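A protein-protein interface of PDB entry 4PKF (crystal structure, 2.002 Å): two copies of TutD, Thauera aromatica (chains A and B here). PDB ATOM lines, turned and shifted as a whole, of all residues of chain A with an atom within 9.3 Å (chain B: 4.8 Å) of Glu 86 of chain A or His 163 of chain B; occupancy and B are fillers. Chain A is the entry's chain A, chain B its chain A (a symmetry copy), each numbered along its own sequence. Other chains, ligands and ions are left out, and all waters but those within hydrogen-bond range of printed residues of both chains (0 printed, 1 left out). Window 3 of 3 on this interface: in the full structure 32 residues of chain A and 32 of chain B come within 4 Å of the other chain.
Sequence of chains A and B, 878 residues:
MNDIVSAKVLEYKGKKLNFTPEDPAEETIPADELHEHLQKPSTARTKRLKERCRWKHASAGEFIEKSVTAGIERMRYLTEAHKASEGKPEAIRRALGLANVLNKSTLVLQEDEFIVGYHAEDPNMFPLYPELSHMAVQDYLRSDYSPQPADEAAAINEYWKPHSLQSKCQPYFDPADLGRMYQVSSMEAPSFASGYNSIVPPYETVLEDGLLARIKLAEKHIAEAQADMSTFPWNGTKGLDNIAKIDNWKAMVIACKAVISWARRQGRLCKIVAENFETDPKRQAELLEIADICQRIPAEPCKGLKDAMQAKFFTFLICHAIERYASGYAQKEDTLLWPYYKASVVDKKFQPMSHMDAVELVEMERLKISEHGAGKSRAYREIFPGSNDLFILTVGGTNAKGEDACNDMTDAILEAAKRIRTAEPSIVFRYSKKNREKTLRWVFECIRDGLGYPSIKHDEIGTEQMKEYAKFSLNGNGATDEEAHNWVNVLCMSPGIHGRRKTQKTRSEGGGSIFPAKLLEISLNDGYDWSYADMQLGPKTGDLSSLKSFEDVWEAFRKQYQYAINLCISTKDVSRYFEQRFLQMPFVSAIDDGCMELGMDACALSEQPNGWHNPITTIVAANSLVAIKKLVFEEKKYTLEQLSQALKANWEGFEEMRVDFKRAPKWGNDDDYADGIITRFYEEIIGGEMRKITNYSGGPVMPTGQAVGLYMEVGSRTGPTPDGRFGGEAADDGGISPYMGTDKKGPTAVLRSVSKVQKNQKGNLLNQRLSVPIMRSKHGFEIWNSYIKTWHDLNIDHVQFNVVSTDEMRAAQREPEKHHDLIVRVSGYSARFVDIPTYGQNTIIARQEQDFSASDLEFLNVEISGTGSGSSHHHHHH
Among the printed residues, merely in contact across the chains: His 163 of chain A with Glu 86 of chain B (3.3 Å), Glu 86 of chain A with His 163 of chain B (3.3 Å), Gly 87 of chain A with Pro 162 of chain B (3.5 Å), Gly 87 of chain A with Lys 168 of chain B (3.6 Å), Glu 86 of chain A with Pro 162 of chain B (3.9 Å) and Pro 162 of chain A with Glu 86 of chain B (3.9 Å).
Of the 20 printed residues of chain A, 4 touch a printed residue of chain B.
Hydrophobic or aromatic side chains of chain A within 4 Å of the printed part of chain B: Pro 162 and His 163.
Printed residues of chain B that touch a printed residue of chain A: Glu 86, Pro 162, His 163 and Lys 168.
Among the printed residues, 6 pairs touch across the chains.
Among the printed residues, no Asp or Glu carboxylate lies within 4 Å of a Lys or Arg side-chain nitrogen of the other chain.
Glu 86 of chain A touches Pro 162 of chain B, and with the chains exchanged Pro 162 of chain A touches Glu 86 of chain B.
Glu 86 of chain A touches His 163 of chain B, and with the chains exchanged His 163 of chain A touches Glu 86 of chain B.
The guanidinium group (NH2) of Arg 93 of chain A is in salt-bridge range of the side-chain carboxylate (OE1) of Glu 86 of chain A (3.3 Å).
Glu 86 of chain A touches just these residues of chain B: Pro 162 (3.9 Å) and His 163 (3.3 Å).
Of the printed residues of chain B, Gly 87 of chain A touches Pro 162 and Lys 168.
Glu 90 of chain A touches none of the printed residues of chain B.
Ile 92 of chain A touches none of the printed residues of chain B.
Of the printed residues of chain B, Pro 162 of chain A touches Glu 86.
Of the printed residues of chain B, His 163 of chain A touches Glu 86.
Of the printed residues of chain A, Glu 86 of chain B touches Pro 162 (3.9 Å) and His 163 (3.3 Å).
Pro 162 of chain B touches just these residues of chain A: Glu 86 (3.9 Å) and Gly 87 (3.5 Å).
No residue of chain A comes within 4 Å of Ser 164 of chain B.
Of the printed residues of chain A, Lys 168 of chain B touches Gly 87 (3.6 Å).
The nearest residue of chain B that does not touch Glu 86 of chain A is Glu 86 of chain B (4.1 Å).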
ATOM      1  N   THR A  79      -1.971 -28.586  32.015  1.00  0.00           N
ATOM      2  CA  THR A  79      -1.086 -27.507  32.436  1.00  0.00           C
ATOM      3  C   THR A  79       0.128 -27.369  31.516  1.00  0.00           C
ATOM      4  O   THR A  79       0.474 -26.273  31.085  1.00  0.00           O
ATOM      5  CB  THR A  79      -0.626 -27.730  33.892  1.00  0.00           C
ATOM      6  OG1 THR A  79      -1.779 -27.802  34.735  1.00  0.00           O
ATOM      7  CG2 THR A  79       0.262 -26.586  34.384  1.00  0.00           C
ATOM      8  N   GLU A  80       0.746 -28.498  31.185  1.00  0.00           N
ATOM      9  CA  GLU A  80       1.918 -28.496  30.323  1.00  0.00           C
ATOM     10  C   GLU A  80       1.560 -27.880  28.981  1.00  0.00           C
ATOM     11  O   GLU A  80       2.287 -27.048  28.455  1.00  0.00           O
ATOM     12  CB  GLU A  80       2.448 -29.922  30.164  1.00  0.00           C
ATOM     13  CG  GLU A  80       3.614 -30.080  29.216  1.00  0.00           C
ATOM     14  CD  GLU A  80       4.029 -31.553  29.054  1.00  0.00           C
ATOM     15  OE1 GLU A  80       5.226 -31.842  29.287  1.00  0.00           O
ATOM     16  OE2 GLU A  80       3.167 -32.416  28.708  1.00  0.00           O
ATOM     17  N   ALA A  81       0.404 -28.256  28.447  1.00  0.00           N
ATOM     18  CA  ALA A  81      -0.034 -27.728  27.159  1.00  0.00           C
ATOM     19  C   ALA A  81      -0.339 -26.230  27.226  1.00  0.00           C
ATOM     20  O   ALA A  81      -0.042 -25.484  26.308  1.00  0.00           O
ATOM     21  CB  ALA A  81      -1.264 -28.502  26.667  1.00  0.00           C
ATOM     22  N   HIS A  82      -0.951 -25.801  28.316  1.00  0.00           N
ATOM     23  CA  HIS A  82      -1.350 -24.411  28.447  1.00  0.00           C
ATOM     24  C   HIS A  82      -0.120 -23.508  28.480  1.00  0.00           C
ATOM     25  O   HIS A  82      -0.121 -22.436  27.886  1.00  0.00           O
ATOM     26  CB  HIS A  82      -2.186 -24.212  29.707  1.00  0.00           C
ATOM     27  CG  HIS A  82      -2.949 -22.920  29.733  1.00  0.00           C
ATOM     28  ND1 HIS A  82      -2.589 -21.855  30.536  1.00  0.00           N
ATOM     29  CD2 HIS A  82      -4.056 -22.526  29.055  1.00  0.00           C
ATOM     30  CE1 HIS A  82      -3.461 -20.873  30.371  1.00  0.00           C
ATOM     31  NE2 HIS A  82      -4.357 -21.251  29.472  1.00  0.00           N
ATOM     32  N   LYS A  83       0.925 -23.951  29.167  1.00  0.00           N
ATOM     33  CA  LYS A  83       2.156 -23.157  29.239  1.00  0.00           C
ATOM     34  C   LYS A  83       2.810 -23.047  27.879  1.00  0.00           C
ATOM     35  O   LYS A  83       3.307 -21.983  27.514  1.00  0.00           O
ATOM     36  CB  LYS A  83       3.129 -23.766  30.243  1.00  0.00           C
ATOM     37  CG  LYS A  83       2.674 -23.581  31.679  1.00  0.00           C
ATOM     38  CD  LYS A  83       3.497 -24.412  32.649  1.00  0.00           C
ATOM     39  CE  LYS A  83       3.170 -24.020  34.069  1.00  0.00           C
ATOM     40  NZ  LYS A  83       3.541 -25.084  35.061  1.00  0.00           N
ATOM     41  N   ALA A  84       2.776 -24.146  27.125  1.00  0.00           N
ATOM     42  CA  ALA A  84       3.436 -24.237  25.836  1.00  0.00           C
ATOM     43  C   ALA A  84       2.678 -23.480  24.765  1.00  0.00           C
ATOM     44  O   ALA A  84       3.264 -23.104  23.766  1.00  0.00           O
ATOM     45  CB  ALA A  84       3.599 -25.689  25.415  1.00  0.00           C
ATOM     46  N   SER A  85       1.381 -23.250  24.958  1.00  0.00           N
ATOM     47  CA  SER A  85       0.573 -22.666  23.885  1.00  0.00           C
ATOM     48  C   SER A  85       0.311 -21.172  24.052  1.00  0.00           C
ATOM     49  O   SER A  85      -0.495 -20.618  23.302  1.00  0.00           O
ATOM     50  CB  SER A  85      -0.774 -23.399  23.778  1.00  0.00           C
ATOM     51  OG  SER A  85      -1.556 -23.091  24.927  1.00  0.00           O
ATOM     52  N   GLU A  86       0.958 -20.518  25.022  1.00  0.00           N
ATOM     53  CA  GLU A  86       0.777 -19.066  25.211  1.00  0.00           C
ATOM     54  C   GLU A  86       0.925 -18.299  23.883  1.00  0.00           C
ATOM     55  O   GLU A  86       1.752 -18.637  23.049  1.00  0.00           O
ATOM     56  CB  GLU A  86       1.776 -18.502  26.256  1.00  0.00           C
ATOM     57  CG  GLU A  86       1.329 -18.663  27.730  1.00  0.00           C
ATOM     58  CD  GLU A  86       0.078 -17.815  28.107  1.00  0.00           C
ATOM     59  OE1 GLU A  86      -0.606 -18.115  29.147  1.00  0.00           O
ATOM     60  OE2 GLU A  86      -0.227 -16.846  27.367  1.00  0.00           O
ATOM     61  N   GLY A  87       0.067 -17.310  23.680  1.00  0.00           N
ATOM     62  CA  GLY A  87       0.041 -16.537  22.458  1.00  0.00           C
ATOM     63  C   GLY A  87      -0.856 -17.063  21.333  1.00  0.00           C
ATOM     64  O   GLY A  87      -1.307 -16.272  20.509  1.00  0.00           O
ATOM     65  N   LYS A  88      -1.116 -18.377  21.283  1.00  0.00           N
ATOM     66  CA  LYS A  88      -1.921 -18.986  20.197  1.00  0.00           C
ATOM     67  C   LYS A  88      -3.422 -18.672  20.388  1.00  0.00           C
ATOM     68  O   LYS A  88      -3.831 -18.280  21.468  1.00  0.00           O
ATOM     69  CB  LYS A  88      -1.689 -20.513  20.144  1.00  0.00           C
ATOM     70  CG  LYS A  88      -0.261 -20.918  19.755  1.00  0.00           C
ATOM     71  CD  LYS A  88      -0.186 -22.389  19.462  1.00  0.00           C
ATOM     72  CE  LYS A  88       1.225 -22.923  19.562  1.00  0.00           C
ATOM     73  NZ  LYS A  88       2.045 -22.331  18.481  1.00  0.00           N
ATOM     74  N   PRO A  89      -4.235 -18.794  19.327  1.00  0.00           N
ATOM     75  CA  PRO A  89      -5.650 -18.455  19.506  1.00  0.00           C
ATOM     76  C   PRO A  89      -6.294 -19.398  20.536  1.00  0.00           C
ATOM     77  O   PRO A  89      -5.909 -20.551  20.568  1.00  0.00           O
ATOM     78  CB  PRO A  89      -6.252 -18.696  18.131  1.00  0.00           C
ATOM     79  CG  PRO A  89      -5.072 -18.529  17.154  1.00  0.00           C
ATOM     80  CD  PRO A  89      -3.861 -18.982  17.910  1.00  0.00           C
ATOM     81  N   GLU A  90      -7.242 -18.926  21.327  1.00  0.00           N
ATOM     82  CA  GLU A  90      -7.734 -19.699  22.469  1.00  0.00           C
ATOM     83  C   GLU A  90      -8.351 -21.020  22.039  1.00  0.00           C
ATOM     84  O   GLU A  90      -8.195 -22.034  22.738  1.00  0.00           O
ATOM     85  CB  GLU A  90      -8.752 -18.891  23.253  1.00  0.00           C
ATOM     86  CG  GLU A  90      -8.176 -17.652  23.972  1.00  0.00           C
ATOM     87  CD  GLU A  90      -7.146 -17.990  25.049  1.00  0.00           C
ATOM     88  OE1 GLU A  90      -6.394 -17.070  25.434  1.00  0.00           O
ATOM     89  OE2 GLU A  90      -7.087 -19.151  25.546  1.00  0.00           O
ATOM     90  N   ILE A  92      -7.542 -22.877  19.568  1.00  0.00           N
ATOM     91  CA  ILE A  92      -6.423 -23.759  19.269  1.00  0.00           C
ATOM     92  C   ILE A  92      -5.722 -24.188  20.556  1.00  0.00           C
ATOM     93  O   ILE A  92      -5.344 -25.345  20.698  1.00  0.00           O
ATOM     94  CB  ILE A  92      -5.427 -23.070  18.300  1.00  0.00           C
ATOM     95  CG1 ILE A  92      -6.060 -23.019  16.906  1.00  0.00           C
ATOM     96  CG2 ILE A  92      -4.074 -23.806  18.279  1.00  0.00           C
ATOM     97  CD1 ILE A  92      -5.253 -22.260  15.872  1.00  0.00           C
ATOM     98  N   ARG A  93      -5.544 -23.262  21.497  1.00  0.00           N
ATOM     99  CA  ARG A  93      -5.014 -23.637  22.816  1.00  0.00           C
ATOM    100  C   ARG A  93      -5.841 -24.732  23.471  1.00  0.00           C
ATOM    101  O   ARG A  93      -5.288 -25.638  24.075  1.00  0.00           O
ATOM    102  CB  ARG A  93      -4.957 -22.429  23.752  1.00  0.00           C
ATOM    103  CG  ARG A  93      -4.075 -21.289  23.179  1.00  0.00           C
ATOM    104  CD  ARG A  93      -3.944 -20.220  24.203  1.00  0.00           C
ATOM    105  NE  ARG A  93      -3.074 -20.651  25.300  1.00  0.00           N
ATOM    106  CZ  ARG A  93      -2.956 -19.996  26.453  1.00  0.00           C
ATOM    107  NH1 ARG A  93      -3.673 -18.905  26.665  1.00  0.00           N
ATOM    108  NH2 ARG A  93      -2.122 -20.421  27.391  1.00  0.00           N
ATOM    109  N   ARG A  94      -7.162 -24.650  23.347  1.00  0.00           N
ATOM    110  CA  ARG A  94      -8.023 -25.647  23.962  1.00  0.00           C
ATOM    111  C   ARG A  94      -7.853 -27.007  23.264  1.00  0.00           C
ATOM    112  O   ARG A  94      -7.786 -28.055  23.916  1.00  0.00           O
ATOM    113  CB  ARG A  94      -9.490 -25.166  23.938  1.00  0.00           C
ATOM    114  CG  ARG A  94      -9.793 -24.048  24.973  1.00  0.00           C
ATOM    115  CD  ARG A  94     -10.034 -24.645  26.354  1.00  0.00           C
ATOM    116  NE  ARG A  94     -11.215 -25.501  26.361  1.00  0.00           N
ATOM    117  CZ  ARG A  94     -11.593 -26.275  27.375  1.00  0.00           C
ATOM    118  NH1 ARG A  94     -12.702 -26.992  27.266  1.00  0.00           N
ATOM    119  NH2 ARG A  94     -10.891 -26.316  28.497  1.00  0.00           N
ATOM    120  N   LEU A  96      -5.176 -28.072  21.729  1.00  0.00           N
ATOM    121  CA  LEU A  96      -3.852 -28.545  22.071  1.00  0.00           C
ATOM    122  C   LEU A  96      -3.853 -29.146  23.474  1.00  0.00           C
ATOM    123  O   LEU A  96      -3.190 -30.157  23.718  1.00  0.00           O
ATOM    124  CB  LEU A  96      -2.845 -27.397  21.972  1.00  0.00           C
ATOM    125  CG  LEU A  96      -2.455 -26.995  20.530  1.00  0.00           C
ATOM    126  CD1 LEU A  96      -1.639 -25.706  20.562  1.00  0.00           C
ATOM    127  CD2 LEU A  96      -1.731 -28.136  19.799  1.00  0.00           C
ATOM    128  N   TYR A 159      -1.304 -22.252  39.498  1.00  0.00           N
ATOM    129  CA  TYR A 159      -1.055 -21.794  38.131  1.00  0.00           C
ATOM    130  C   TYR A 159      -2.364 -21.421  37.430  1.00  0.00           C
ATOM    131  O   TYR A 159      -2.436 -20.404  36.755  1.00  0.00           O
ATOM    132  CB  TYR A 159      -0.303 -22.851  37.314  1.00  0.00           C
ATOM    133  CG  TYR A 159      -0.310 -22.532  35.837  1.00  0.00           C
ATOM    134  CD1 TYR A 159       0.617 -21.645  35.294  1.00  0.00           C
ATOM    135  CD2 TYR A 159      -1.272 -23.083  34.992  1.00  0.00           C
ATOM    136  CE1 TYR A 159       0.594 -21.323  33.937  1.00  0.00           C
ATOM    137  CE2 TYR A 159      -1.309 -22.772  33.649  1.00  0.00           C
ATOM    138  CZ  TYR A 159      -0.368 -21.891  33.118  1.00  0.00           C
ATOM    139  OH  TYR A 159      -0.392 -21.582  31.766  1.00  0.00           O
ATOM    140  N   TRP A 160      -3.402 -22.242  37.583  1.00  0.00           N
ATOM    141  CA  TRP A 160      -4.639 -22.042  36.831  1.00  0.00           C
ATOM    142  C   TRP A 160      -5.523 -20.944  37.440  1.00  0.00           C
ATOM    143  O   TRP A 160      -6.372 -20.381  36.751  1.00  0.00           O
ATOM    144  CB  TRP A 160      -5.443 -23.362  36.748  1.00  0.00           C
ATOM    145  CG  TRP A 160      -4.951 -24.266  35.637  1.00  0.00           C
ATOM    146  CD1 TRP A 160      -4.069 -25.300  35.744  1.00  0.00           C
ATOM    147  CD2 TRP A 160      -5.286 -24.163  34.254  1.00  0.00           C
ATOM    148  NE1 TRP A 160      -3.871 -25.887  34.507  1.00  0.00           N
ATOM    149  CE2 TRP A 160      -4.614 -25.203  33.578  1.00  0.00           C
ATOM    150  CE3 TRP A 160      -6.138 -23.313  33.522  1.00  0.00           C
ATOM    151  CZ2 TRP A 160      -4.732 -25.399  32.199  1.00  0.00           C
ATOM    152  CZ3 TRP A 160      -6.259 -23.511  32.168  1.00  0.00           C
ATOM    153  CH2 TRP A 160      -5.549 -24.539  31.513  1.00  0.00           C
ATOM    154  N   PRO A 162      -5.615 -17.715  38.216  1.00  0.00           N
ATOM    155  CA  PRO A 162      -5.952 -16.470  37.504  1.00  0.00           C
ATOM    156  C   PRO A 162      -6.627 -16.695  36.138  1.00  0.00           C
ATOM    157  O   PRO A 162      -7.268 -15.796  35.601  1.00  0.00           O
ATOM    158  CB  PRO A 162      -4.587 -15.791  37.315  1.00  0.00           C
ATOM    159  CG  PRO A 162      -3.601 -16.893  37.385  1.00  0.00           C
ATOM    160  CD  PRO A 162      -4.157 -17.830  38.426  1.00  0.00           C
ATOM    161  N   HIS A 163      -6.482 -17.902  35.597  1.00  0.00           N
ATOM    162  CA  HIS A 163      -7.032 -18.254  34.273  1.00  0.00           C
ATOM    163  C   HIS A 163      -8.367 -19.003  34.349  1.00  0.00           C
ATOM    164  O   HIS A 163      -8.983 -19.311  33.326  1.00  0.00           O
ATOM    165  CB  HIS A 163      -6.046 -19.133  33.513  1.00  0.00           C
ATOM    166  CG  HIS A 163      -4.740 -18.474  33.245  1.00  0.00           C
ATOM    167  ND1 HIS A 163      -4.604 -17.440  32.344  1.00  0.00           N
ATOM    168  CD2 HIS A 163      -3.511 -18.694  33.762  1.00  0.00           C
ATOM    169  CE1 HIS A 163      -3.339 -17.060  32.308  1.00  0.00           C
ATOM    170  NE2 HIS A 163      -2.661 -17.786  33.178  1.00  0.00           N
ATOM    171  N   HIS B  82       2.917  -6.897  32.396  1.00  0.00           N
ATOM    172  CA  HIS B  82       2.272  -7.931  31.607  1.00  0.00           C
ATOM    173  C   HIS B  82       2.287  -9.259  32.360  1.00  0.00           C
ATOM    174  O   HIS B  82       1.310  -9.996  32.336  1.00  0.00           O
ATOM    175  CB  HIS B  82       2.965  -8.081  30.257  1.00  0.00           C
ATOM    176  CG  HIS B  82       2.160  -8.839  29.241  1.00  0.00           C
ATOM    177  ND1 HIS B  82       2.466 -10.131  28.859  1.00  0.00           N
ATOM    178  CD2 HIS B  82       1.063  -8.482  28.528  1.00  0.00           C
ATOM    179  CE1 HIS B  82       1.606 -10.523  27.930  1.00  0.00           C
ATOM    180  NE2 HIS B  82       0.740  -9.544  27.718  1.00  0.00           N
ATOM    181  N   GLU B  86      -1.594 -11.292  34.048  1.00  0.00           N
ATOM    182  CA  GLU B  86      -2.148 -12.494  33.396  1.00  0.00           C
ATOM    183  C   GLU B  86      -3.553 -12.833  33.930  1.00  0.00           C
ATOM    184  O   GLU B  86      -3.831 -12.682  35.110  1.00  0.00           O
ATOM    185  CB  GLU B  86      -1.211 -13.718  33.572  1.00  0.00           C
ATOM    186  CG  GLU B  86      -0.054 -13.800  32.547  1.00  0.00           C
ATOM    187  CD  GLU B  86      -0.522 -14.061  31.084  1.00  0.00           C
ATOM    188  OE1 GLU B  86       0.260 -13.795  30.107  1.00  0.00           O
ATOM    189  OE2 GLU B  86      -1.673 -14.534  30.907  1.00  0.00           O
ATOM    190  N   GLU B 131       6.094  -5.120  22.292  1.00  0.00           N
ATOM    191  CA  GLU B 131       4.754  -5.690  22.127  1.00  0.00           C
ATOM    192  C   GLU B 131       4.322  -5.665  20.650  1.00  0.00           C
ATOM    193  O   GLU B 131       3.273  -6.231  20.292  1.00  0.00           O
ATOM    194  CB  GLU B 131       3.739  -4.923  23.001  1.00  0.00           C
ATOM    195  CG  GLU B 131       3.405  -3.491  22.538  1.00  0.00           C
ATOM    196  CD  GLU B 131       4.473  -2.416  22.919  1.00  0.00           C
ATOM    197  OE1 GLU B 131       5.627  -2.748  23.236  1.00  0.00           O
ATOM    198  OE2 GLU B 131       4.137  -1.222  22.894  1.00  0.00           O
ATOM    199  N   TYR B 159      10.526 -12.919  25.794  1.00  0.00           N
ATOM    200  CA  TYR B 159       9.260 -13.030  26.520  1.00  0.00           C
ATOM    201  C   TYR B 159       8.089 -12.558  25.655  1.00  0.00           C
ATOM    202  O   TYR B 159       7.045 -13.195  25.626  1.00  0.00           O
ATOM    203  CB  TYR B 159       9.296 -12.242  27.833  1.00  0.00           C
ATOM    204  CG  TYR B 159       7.920 -12.089  28.438  1.00  0.00           C
ATOM    205  CD1 TYR B 159       7.365 -13.103  29.215  1.00  0.00           C
ATOM    206  CD2 TYR B 159       7.154 -10.950  28.193  1.00  0.00           C
ATOM    207  CE1 TYR B 159       6.082 -12.980  29.747  1.00  0.00           C
ATOM    208  CE2 TYR B 159       5.883 -10.814  28.710  1.00  0.00           C
ATOM    209  CZ  TYR B 159       5.346 -11.833  29.496  1.00  0.00           C
ATOM    210  OH  TYR B 159       4.072 -11.700  30.029  1.00  0.00           O
ATOM    211  N   TRP B 160       8.252 -11.439  24.950  1.00  0.00           N
ATOM    212  CA  TRP B 160       7.139 -10.838  24.219  1.00  0.00           C
ATOM    213  C   TRP B 160       6.869 -11.543  22.882  1.00  0.00           C
ATOM    214  O   TRP B 160       5.770 -11.441  22.340  1.00  0.00           O
ATOM    215  CB  TRP B 160       7.407  -9.335  23.963  1.00  0.00           C
ATOM    216  CG  TRP B 160       7.045  -8.475  25.156  1.00  0.00           C
ATOM    217  CD1 TRP B 160       7.882  -8.028  26.135  1.00  0.00           C
ATOM    218  CD2 TRP B 160       5.738  -8.019  25.504  1.00  0.00           C
ATOM    219  NE1 TRP B 160       7.179  -7.268  27.053  1.00  0.00           N
ATOM    220  CE2 TRP B 160       5.859  -7.249  26.680  1.00  0.00           C
ATOM    221  CE3 TRP B 160       4.473  -8.148  24.899  1.00  0.00           C
ATOM    222  CZ2 TRP B 160       4.759  -6.638  27.290  1.00  0.00           C
ATOM    223  CZ3 TRP B 160       3.395  -7.540  25.496  1.00  0.00           C
ATOM    224  CH2 TRP B 160       3.539  -6.803  26.691  1.00  0.00           C
ATOM    225  N   LYS B 161       7.866 -12.230  22.341  1.00  0.00           N
ATOM    226  CA  LYS B 161       7.734 -12.712  20.956  1.00  0.00           C
ATOM    227  C   LYS B 161       6.407 -13.467  20.685  1.00  0.00           C
ATOM    228  O   LYS B 161       5.713 -13.120  19.735  1.00  0.00           O
ATOM    229  CB  LYS B 161       8.940 -13.573  20.551  1.00  0.00           C
ATOM    230  CG  LYS B 161       8.882 -14.060  19.081  1.00  0.00           C
ATOM    231  CD  LYS B 161      10.159 -14.766  18.638  1.00  0.00           C
ATOM    232  CE  LYS B 161       9.880 -15.573  17.330  1.00  0.00           C
ATOM    233  NZ  LYS B 161      11.137 -16.146  16.781  1.00  0.00           N
ATOM    234  N   PRO B 162       6.033 -14.455  21.520  1.00  0.00           N
ATOM    235  CA  PRO B 162       4.772 -15.155  21.223  1.00  0.00           C
ATOM    236  C   PRO B 162       3.518 -14.273  21.372  1.00  0.00           C
ATOM    237  O   PRO B 162       2.460 -14.593  20.837  1.00  0.00           O
ATOM    238  CB  PRO B 162       4.747 -16.291  22.258  1.00  0.00           C
ATOM    239  CG  PRO B 162       5.617 -15.822  23.359  1.00  0.00           C
ATOM    240  CD  PRO B 162       6.728 -15.074  22.668  1.00  0.00           C
ATOM    241  N   HIS B 163       3.657 -13.162  22.092  1.00  0.00           N
ATOM    242  CA  HIS B 163       2.535 -12.242  22.361  1.00  0.00           C
ATOM    243  C   HIS B 163       2.507 -11.027  21.425  1.00  0.00           C
ATOM    244  O   HIS B 163       1.596 -10.199  21.484  1.00  0.00           O
ATOM    245  CB  HIS B 163       2.614 -11.725  23.793  1.00  0.00           C
ATOM    246  CG  HIS B 163       2.512 -12.794  24.821  1.00  0.00           C
ATOM    247  ND1 HIS B 163       1.340 -13.475  25.067  1.00  0.00           N
ATOM    248  CD2 HIS B 163       3.437 -13.308  25.663  1.00  0.00           C
ATOM    249  CE1 HIS B 163       1.544 -14.356  26.031  1.00  0.00           C
ATOM    250  NE2 HIS B 163       2.813 -14.293  26.390  1.00  0.00           N
ATOM    251  N   SER B 164       3.535 -10.893  20.607  1.00  0.00           N
ATOM    252  CA  SER B 164       3.701  -9.657  19.827  1.00  0.00           C
ATOM    253  C   SER B 164       2.623  -9.544  18.754  1.00  0.00           C
ATOM    254  O   SER B 164       2.097 -10.560  18.247  1.00  0.00           O
ATOM    255  CB  SER B 164       5.108  -9.613  19.195  1.00  0.00           C
ATOM    256  OG  SER B 164       5.207 -10.552  18.136  1.00  0.00           O
ATOM    257  N   LEU B 165       2.309  -8.308  18.374  1.00  0.00           N
ATOM    258  CA  LEU B 165       1.355  -8.073  17.291  1.00  0.00           C
ATOM    259  C   LEU B 165       1.832  -8.801  16.032  1.00  0.00           C
ATOM    260  O   LEU B 165       1.044  -9.411  15.298  1.00  0.00           O
ATOM    261  CB  LEU B 165       1.186  -6.570  17.035  1.00  0.00           C
ATOM    262  CG  LEU B 165       0.180  -6.157  15.954  1.00  0.00           C
ATOM    263  CD1 LEU B 165      -1.219  -6.613  16.339  1.00  0.00           C
ATOM    264  CD2 LEU B 165       0.186  -4.653  15.706  1.00  0.00           C
ATOM    265  N   LYS B 168       0.882 -12.408  16.296  1.00  0.00           N
ATOM    266  CA  LYS B 168      -0.551 -12.633  16.168  1.00  0.00           C
ATOM    267  C   LYS B 168      -1.035 -12.616  14.713  1.00  0.00           C
ATOM    268  O   LYS B 168      -1.948 -13.342  14.365  1.00  0.00           O
ATOM    269  CB  LYS B 168      -1.322 -11.585  16.975  1.00  0.00           C
ATOM    270  CG  LYS B 168      -0.964 -11.673  18.436  1.00  0.00           C
ATOM    271  CD  LYS B 168      -2.013 -11.104  19.316  1.00  0.00           C
ATOM    272  CE  LYS B 168      -1.703 -11.420  20.795  1.00  0.00           C
ATOM    273  NZ  LYS B 168      -1.963 -12.832  21.100  1.00  0.00           N
